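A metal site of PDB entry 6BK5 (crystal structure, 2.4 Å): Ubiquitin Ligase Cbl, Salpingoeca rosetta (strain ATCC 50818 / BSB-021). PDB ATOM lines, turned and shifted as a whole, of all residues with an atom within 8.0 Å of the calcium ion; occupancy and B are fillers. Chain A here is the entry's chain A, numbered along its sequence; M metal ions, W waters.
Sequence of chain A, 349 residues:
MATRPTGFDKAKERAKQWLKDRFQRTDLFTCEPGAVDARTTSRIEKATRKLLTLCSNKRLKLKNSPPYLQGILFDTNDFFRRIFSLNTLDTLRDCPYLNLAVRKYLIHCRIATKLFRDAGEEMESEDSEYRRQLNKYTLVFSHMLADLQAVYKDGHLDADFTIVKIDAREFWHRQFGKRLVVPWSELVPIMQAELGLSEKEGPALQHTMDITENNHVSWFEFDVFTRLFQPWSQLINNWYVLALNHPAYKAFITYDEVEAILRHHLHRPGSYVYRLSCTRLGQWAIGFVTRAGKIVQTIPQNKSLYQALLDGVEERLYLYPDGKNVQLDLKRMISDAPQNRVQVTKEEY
The side-chain carboxylate of Glu 221 lies close to the backbone NH of Ile 211 (3.1 Å).
The backbone NH of Glu 213 lies close to the side-chain carboxylate of Asp 210, at 2.8 Å.
The side-chain hydroxyl of Ser 218 is in hydrogen-bond range of the backbone NH of Glu 221, at 3.1 Å.
The side-chain carboxylate (OD2) of Asp 210 sits at hydrogen-bond distance from the side-chain amide nitrogen (NE2) of Gln 206 (3.0 Å).
OD2 of Asp 210 is in hydrogen-bond range of N of Asn 215 (2.9 Å).
The side-chain amino group (NZ) of Lys 104 sits close to the backbone carbonyl oxygen (O) of Thr 212.
Along chain A the residues within 4 Å of the calcium ion span positions 210 to 221.
The nearest printed residue that does not touch the calcium ion is Glu 213 (4.01 Å).
The calcium ion is bound by OD1 of Asp 210, 2.3 Å away.
OE1 of Glu 221 is bound to the calcium ion (2.4 Å).
The backbone carbonyl oxygen (O) of His 216 is bound to the calcium ion (2.5 Å).
The side-chain amide oxygen (OD1) of Asn 214 binds the calcium ion (2.5 Å).
The calcium ion is bound by the side-chain hydroxyl (OG1) of Thr 212 (2.5 Å).
The calcium ion is bound by OE2 of Glu 221 (2.6 Å).
Water W1 lies within hydrogen-bond range of the side-chain carboxylate (OD2) of Asp 147 (2.7 Å) and the side-chain amide nitrogen (ND2) of Asn 214 (3.0 Å).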
ATOM      1  N   TYR A  97     -22.405  23.293  10.279  1.00  0.00           N
ATOM      2  CA  TYR A  97     -21.606  24.195   9.465  1.00  0.00           C
ATOM      3  C   TYR A  97     -21.047  25.358  10.278  1.00  0.00           C
ATOM      4  O   TYR A  97     -19.856  25.685  10.164  1.00  0.00           O
ATOM      5  CB  TYR A  97     -22.395  24.757   8.277  1.00  0.00           C
ATOM      6  CG  TYR A  97     -21.476  25.652   7.478  1.00  0.00           C
ATOM      7  CD1 TYR A  97     -20.591  25.109   6.568  1.00  0.00           C
ATOM      8  CD2 TYR A  97     -21.418  27.015   7.707  1.00  0.00           C
ATOM      9  CE1 TYR A  97     -19.719  25.894   5.863  1.00  0.00           C
ATOM     10  CE2 TYR A  97     -20.540  27.810   7.015  1.00  0.00           C
ATOM     11  CZ  TYR A  97     -19.689  27.244   6.097  1.00  0.00           C
ATOM     12  OH  TYR A  97     -18.817  28.029   5.392  1.00  0.00           O
ATOM     13  N   LEU A 100     -18.125  24.497  12.418  1.00  0.00           N
ATOM     14  CA  LEU A 100     -16.949  24.285  11.587  1.00  0.00           C
ATOM     15  C   LEU A 100     -16.355  25.628  11.124  1.00  0.00           C
ATOM     16  O   LEU A 100     -15.142  25.850  11.212  1.00  0.00           O
ATOM     17  CB  LEU A 100     -17.314  23.418  10.385  1.00  0.00           C
ATOM     18  CG  LEU A 100     -16.209  23.192   9.339  1.00  0.00           C
ATOM     19  CD1 LEU A 100     -15.005  22.467   9.939  1.00  0.00           C
ATOM     20  CD2 LEU A 100     -16.749  22.399   8.168  1.00  0.00           C
ATOM     21  N   LYS A 104     -12.611  27.063  11.911  1.00  0.00           N
ATOM     22  CA  LYS A 104     -11.661  27.301  10.832  1.00  0.00           C
ATOM     23  C   LYS A 104     -11.177  28.744  10.834  1.00  0.00           C
ATOM     24  O   LYS A 104      -9.980  29.001  10.651  1.00  0.00           O
ATOM     25  CB  LYS A 104     -12.310  26.958   9.491  1.00  0.00           C
ATOM     26  CG  LYS A 104     -11.511  27.390   8.258  1.00  0.00           C
ATOM     27  CD  LYS A 104     -10.128  26.737   8.213  1.00  0.00           C
ATOM     28  CE  LYS A 104      -9.296  27.209   7.012  1.00  0.00           C
ATOM     29  NZ  LYS A 104      -8.106  26.356   6.751  1.00  0.00           N
ATOM     30  N   HIS A 143     -12.288  32.500   0.277  1.00  0.00           N
ATOM     31  CA  HIS A 143     -13.179  31.357   0.104  1.00  0.00           C
ATOM     32  C   HIS A 143     -14.047  31.132   1.325  1.00  0.00           C
ATOM     33  O   HIS A 143     -15.220  30.768   1.203  1.00  0.00           O
ATOM     34  CB  HIS A 143     -12.370  30.100  -0.177  1.00  0.00           C
ATOM     35  CG  HIS A 143     -11.490  30.203  -1.377  1.00  0.00           C
ATOM     36  ND1 HIS A 143     -11.740  31.074  -2.417  1.00  0.00           N
ATOM     37  CD2 HIS A 143     -10.364  29.539  -1.706  1.00  0.00           C
ATOM     38  CE1 HIS A 143     -10.816  30.929  -3.337  1.00  0.00           C
ATOM     39  NE2 HIS A 143      -9.961  30.012  -2.939  1.00  0.00           N
ATOM     40  N   MET A 144     -13.476  31.286   2.521  1.00  0.00           N
ATOM     41  CA  MET A 144     -14.238  31.021   3.726  1.00  0.00           C
ATOM     42  C   MET A 144     -15.415  31.981   3.840  1.00  0.00           C
ATOM     43  O   MET A 144     -16.514  31.566   4.215  1.00  0.00           O
ATOM     44  CB  MET A 144     -13.342  31.106   4.962  1.00  0.00           C
ATOM     45  CG  MET A 144     -12.241  30.035   4.992  1.00  0.00           C
ATOM     46  SD  MET A 144     -10.887  30.523   6.106  1.00  0.00           S
ATOM     47  CE  MET A 144     -11.795  31.129   7.507  1.00  0.00           C
ATOM     48  N   ASP A 147     -18.060  31.122   1.324  1.00  0.00           N
ATOM     49  CA  ASP A 147     -18.741  29.922   1.777  1.00  0.00           C
ATOM     50  C   ASP A 147     -19.746  30.257   2.876  1.00  0.00           C
ATOM     51  O   ASP A 147     -20.902  29.809   2.858  1.00  0.00           O
ATOM     52  CB  ASP A 147     -17.727  28.897   2.259  1.00  0.00           C
ATOM     53  CG  ASP A 147     -18.308  27.521   2.363  1.00  0.00           C
ATOM     54  OD1 ASP A 147     -19.028  27.101   1.412  1.00  0.00           O
ATOM     55  OD2 ASP A 147     -18.047  26.847   3.392  1.00  0.00           O
ATOM     56  N   VAL A 181     -22.913  19.995   5.035  1.00  0.00           N
ATOM     57  CA  VAL A 181     -21.463  19.865   4.972  1.00  0.00           C
ATOM     58  C   VAL A 181     -21.124  18.423   5.333  1.00  0.00           C
ATOM     59  O   VAL A 181     -21.753  17.835   6.215  1.00  0.00           O
ATOM     60  CB  VAL A 181     -20.821  20.898   5.921  1.00  0.00           C
ATOM     61  CG1 VAL A 181     -21.231  20.585   7.360  1.00  0.00           C
ATOM     62  CG2 VAL A 181     -19.316  20.966   5.778  1.00  0.00           C
ATOM     63  N   VAL A 182     -20.159  17.846   4.625  1.00  0.00           N
ATOM     64  CA  VAL A 182     -19.754  16.463   4.901  1.00  0.00           C
ATOM     65  C   VAL A 182     -18.232  16.392   5.002  1.00  0.00           C
ATOM     66  O   VAL A 182     -17.519  17.158   4.325  1.00  0.00           O
ATOM     67  CB  VAL A 182     -20.281  15.484   3.838  1.00  0.00           C
ATOM     68  CG1 VAL A 182     -21.755  15.696   3.558  1.00  0.00           C
ATOM     69  CG2 VAL A 182     -19.506  15.599   2.584  1.00  0.00           C
ATOM     70  N   TRP A 184     -14.457  15.173   4.252  1.00  0.00           N
ATOM     71  CA  TRP A 184     -13.791  14.659   3.059  1.00  0.00           C
ATOM     72  C   TRP A 184     -13.755  13.139   3.053  1.00  0.00           C
ATOM     73  O   TRP A 184     -13.978  12.508   2.012  1.00  0.00           O
ATOM     74  CB  TRP A 184     -12.364  15.203   2.971  1.00  0.00           C
ATOM     75  CG  TRP A 184     -11.686  14.760   1.735  1.00  0.00           C
ATOM     76  CD1 TRP A 184     -10.714  13.822   1.627  1.00  0.00           C
ATOM     77  CD2 TRP A 184     -11.979  15.193   0.394  1.00  0.00           C
ATOM     78  NE1 TRP A 184     -10.349  13.653   0.310  1.00  0.00           N
ATOM     79  CE2 TRP A 184     -11.109  14.477  -0.468  1.00  0.00           C
ATOM     80  CE3 TRP A 184     -12.868  16.121  -0.158  1.00  0.00           C
ATOM     81  CZ2 TRP A 184     -11.110  14.658  -1.859  1.00  0.00           C
ATOM     82  CZ3 TRP A 184     -12.869  16.299  -1.538  1.00  0.00           C
ATOM     83  CH2 TRP A 184     -11.988  15.570  -2.373  1.00  0.00           C
ATOM     84  N   GLN A 206      -8.960  16.850  -3.471  1.00  0.00           N
ATOM     85  CA  GLN A 206      -9.266  17.671  -2.305  1.00  0.00           C
ATOM     86  C   GLN A 206      -8.708  19.072  -2.465  1.00  0.00           C
ATOM     87  O   GLN A 206      -9.331  20.059  -2.068  1.00  0.00           O
ATOM     88  CB  GLN A 206      -8.754  17.032  -1.016  1.00  0.00           C
ATOM     89  CG  GLN A 206      -9.157  17.831   0.202  1.00  0.00           C
ATOM     90  CD  GLN A 206      -8.889  17.130   1.545  1.00  0.00           C
ATOM     91  OE1 GLN A 206      -8.214  16.083   1.600  1.00  0.00           O
ATOM     92  NE2 GLN A 206      -9.440  17.699   2.624  1.00  0.00           N
ATOM     93  N   MET A 209     -11.328  20.937  -4.632  1.00  0.00           N
ATOM     94  CA  MET A 209     -12.711  20.992  -4.172  1.00  0.00           C
ATOM     95  C   MET A 209     -12.868  21.565  -2.772  1.00  0.00           C
ATOM     96  O   MET A 209     -13.795  22.330  -2.510  1.00  0.00           O
ATOM     97  CB  MET A 209     -13.330  19.597  -4.200  1.00  0.00           C
ATOM     98  CG  MET A 209     -14.803  19.557  -3.831  1.00  0.00           C
ATOM     99  SD  MET A 209     -15.500  17.897  -4.013  1.00  0.00           S
ATOM    100  CE  MET A 209     -15.122  17.512  -5.715  1.00  0.00           C
ATOM    101  N   ASP A 210     -11.992  21.192  -1.852  1.00  0.00           N
ATOM    102  CA  ASP A 210     -11.994  21.717  -0.487  1.00  0.00           C
ATOM    103  C   ASP A 210     -11.266  23.065  -0.487  1.00  0.00           C
ATOM    104  O   ASP A 210     -10.165  23.237   0.037  1.00  0.00           O
ATOM    105  CB  ASP A 210     -11.358  20.682   0.438  1.00  0.00           C
ATOM    106  CG  ASP A 210     -11.200  21.160   1.871  1.00  0.00           C
ATOM    107  OD1 ASP A 210     -11.781  22.198   2.221  1.00  0.00           O
ATOM    108  OD2 ASP A 210     -10.500  20.490   2.644  1.00  0.00           O
ATOM    109  N   ILE A 211     -11.911  24.057  -1.103  1.00  0.00           N
ATOM    110  CA  ILE A 211     -11.245  25.347  -1.255  1.00  0.00           C
ATOM    111  C   ILE A 211     -11.166  26.096   0.068  1.00  0.00           C
ATOM    112  O   ILE A 211     -10.260  26.918   0.263  1.00  0.00           O
ATOM    113  CB  ILE A 211     -11.922  26.194  -2.354  1.00  0.00           C
ATOM    114  CG1 ILE A 211     -13.410  26.389  -2.070  1.00  0.00           C
ATOM    115  CG2 ILE A 211     -11.725  25.523  -3.694  1.00  0.00           C
ATOM    116  CD1 ILE A 211     -14.115  27.320  -3.056  1.00  0.00           C
ATOM    117  N   THR A 212     -12.077  25.840   1.010  1.00  0.00           N
ATOM    118  CA  THR A 212     -11.929  26.476   2.317  1.00  0.00           C
ATOM    119  C   THR A 212     -10.903  25.768   3.181  1.00  0.00           C
ATOM    120  O   THR A 212     -10.561  26.273   4.268  1.00  0.00           O
ATOM    121  CB  THR A 212     -13.277  26.525   3.057  1.00  0.00           C
ATOM    122  OG1 THR A 212     -13.708  25.205   3.389  1.00  0.00           O
ATOM    123  CG2 THR A 212     -14.369  27.217   2.238  1.00  0.00           C
ATOM    124  N   GLU A 213     -10.394  24.624   2.727  1.00  0.00           N
ATOM    125  CA  GLU A 213      -9.289  23.911   3.376  1.00  0.00           C
ATOM    126  C   GLU A 213      -9.620  23.582   4.836  1.00  0.00           C
ATOM    127  O   GLU A 213      -8.837  23.807   5.740  1.00  0.00           O
ATOM    128  CB  GLU A 213      -7.984  24.720   3.268  1.00  0.00           C
ATOM    129  CG  GLU A 213      -7.613  25.035   1.797  1.00  0.00           C
ATOM    130  CD  GLU A 213      -6.171  25.555   1.601  1.00  0.00           C
ATOM    131  OE1 GLU A 213      -5.416  25.624   2.597  1.00  0.00           O
ATOM    132  OE2 GLU A 213      -5.809  25.882   0.442  1.00  0.00           O
ATOM    133  N   ASN A 214     -10.814  23.031   5.047  1.00  0.00           N
ATOM    134  CA  ASN A 214     -11.233  22.617   6.377  1.00  0.00           C
ATOM    135  C   ASN A 214     -11.596  21.143   6.445  1.00  0.00           C
ATOM    136  O   ASN A 214     -12.297  20.747   7.373  1.00  0.00           O
ATOM    137  CB  ASN A 214     -12.406  23.481   6.859  1.00  0.00           C
ATOM    138  CG  ASN A 214     -13.632  23.391   5.946  1.00  0.00           C
ATOM    139  OD1 ASN A 214     -13.693  22.536   5.062  1.00  0.00           O
ATOM    140  ND2 ASN A 214     -14.611  24.280   6.155  1.00  0.00           N
ATOM    141  N   ASN A 215     -11.139  20.331   5.475  1.00  0.00           N
ATOM    142  CA  ASN A 215     -11.345  18.878   5.454  1.00  0.00           C
ATOM    143  C   ASN A 215     -12.801  18.485   5.268  1.00  0.00           C
ATOM    144  O   ASN A 215     -13.173  17.320   5.519  1.00  0.00           O
ATOM    145  CB  ASN A 215     -10.827  18.202   6.723  1.00  0.00           C
ATOM    146  CG  ASN A 215      -9.394  17.829   6.618  1.00  0.00           C
ATOM    147  OD1 ASN A 215      -8.988  17.131   5.685  1.00  0.00           O
ATOM    148  ND2 ASN A 215      -8.594  18.291   7.584  1.00  0.00           N
ATOM    149  N   HIS A 216     -13.646  19.408   4.862  1.00  0.00           N
ATOM    150  CA  HIS A 216     -15.034  19.118   4.603  1.00  0.00           C
ATOM    151  C   HIS A 216     -15.369  19.674   3.230  1.00  0.00           C
ATOM    152  O   HIS A 216     -14.613  20.457   2.653  1.00  0.00           O
ATOM    153  CB  HIS A 216     -15.932  19.717   5.672  1.00  0.00           C
ATOM    154  CG  HIS A 216     -15.743  19.103   7.023  1.00  0.00           C
ATOM    155  ND1 HIS A 216     -14.567  19.230   7.736  1.00  0.00           N
ATOM    156  CD2 HIS A 216     -16.563  18.330   7.775  1.00  0.00           C
ATOM    157  CE1 HIS A 216     -14.684  18.587   8.888  1.00  0.00           C
ATOM    158  NE2 HIS A 216     -15.882  18.028   8.932  1.00  0.00           N
ATOM    159  N   VAL A 217     -16.511  19.270   2.717  1.00  0.00           N
ATOM    160  CA  VAL A 217     -17.070  19.857   1.516  1.00  0.00           C
ATOM    161  C   VAL A 217     -18.488  20.291   1.864  1.00  0.00           C
ATOM    162  O   VAL A 217     -19.347  19.445   2.141  1.00  0.00           O
ATOM    163  CB  VAL A 217     -17.059  18.880   0.335  1.00  0.00           C
ATOM    164  CG1 VAL A 217     -17.674  19.541  -0.901  1.00  0.00           C
ATOM    165  CG2 VAL A 217     -15.609  18.422   0.054  1.00  0.00           C
ATOM    166  N   SER A 218     -18.716  21.594   1.918  1.00  0.00           N
ATOM    167  CA  SER A 218     -20.064  22.109   2.095  1.00  0.00           C
ATOM    168  C   SER A 218     -20.841  21.972   0.779  1.00  0.00           C
ATOM    169  O   SER A 218     -20.273  21.744  -0.294  1.00  0.00           O
ATOM    170  CB  SER A 218     -20.031  23.575   2.503  1.00  0.00           C
ATOM    171  OG  SER A 218     -19.607  24.381   1.409  1.00  0.00           O
ATOM    172  N   GLU A 221     -19.305  24.419  -1.667  1.00  0.00           N
ATOM    173  CA  GLU A 221     -18.093  23.978  -2.359  1.00  0.00           C
ATOM    174  C   GLU A 221     -18.404  22.947  -3.425  1.00  0.00           C
ATOM    175  O   GLU A 221     -17.794  22.972  -4.503  1.00  0.00           O
ATOM    176  CB  GLU A 221     -17.090  23.419  -1.366  1.00  0.00           C
ATOM    177  CG  GLU A 221     -16.506  24.485  -0.474  1.00  0.00           C
ATOM    178  CD  GLU A 221     -15.695  23.873   0.631  1.00  0.00           C
ATOM    179  OE1 GLU A 221     -14.454  24.080   0.644  1.00  0.00           O
ATOM    180  OE2 GLU A 221     -16.319  23.157   1.449  1.00  0.00           O
ATOM    181  N   PHE A 222     -19.353  22.048  -3.135  1.00  0.00           N
ATOM    182  CA  PHE A 222     -19.735  21.058  -4.122  1.00  0.00           C
ATOM    183  C   PHE A 222     -20.433  21.714  -5.302  1.00  0.00           C
ATOM    184  O   PHE A 222     -20.249  21.305  -6.452  1.00  0.00           O
ATOM    185  CB  PHE A 222     -20.639  20.002  -3.509  1.00  0.00           C
ATOM    186  CG  PHE A 222     -20.794  18.766  -4.360  1.00  0.00           C
ATOM    187  CD1 PHE A 222     -19.741  17.904  -4.548  1.00  0.00           C
ATOM    188  CD2 PHE A 222     -22.009  18.472  -4.953  1.00  0.00           C
ATOM    189  CE1 PHE A 222     -19.887  16.752  -5.316  1.00  0.00           C
ATOM    190  CE2 PHE A 222     -22.169  17.323  -5.710  1.00  0.00           C
ATOM    191  CZ  PHE A 222     -21.098  16.468  -5.895  1.00  0.00           C
HETATM  192 CA    CA M   1     -13.976  22.823   2.610  1.00  0.00          CA
HETATM  193  O   HOH W   1     -16.550  24.701   3.890  1.00  0.00           O
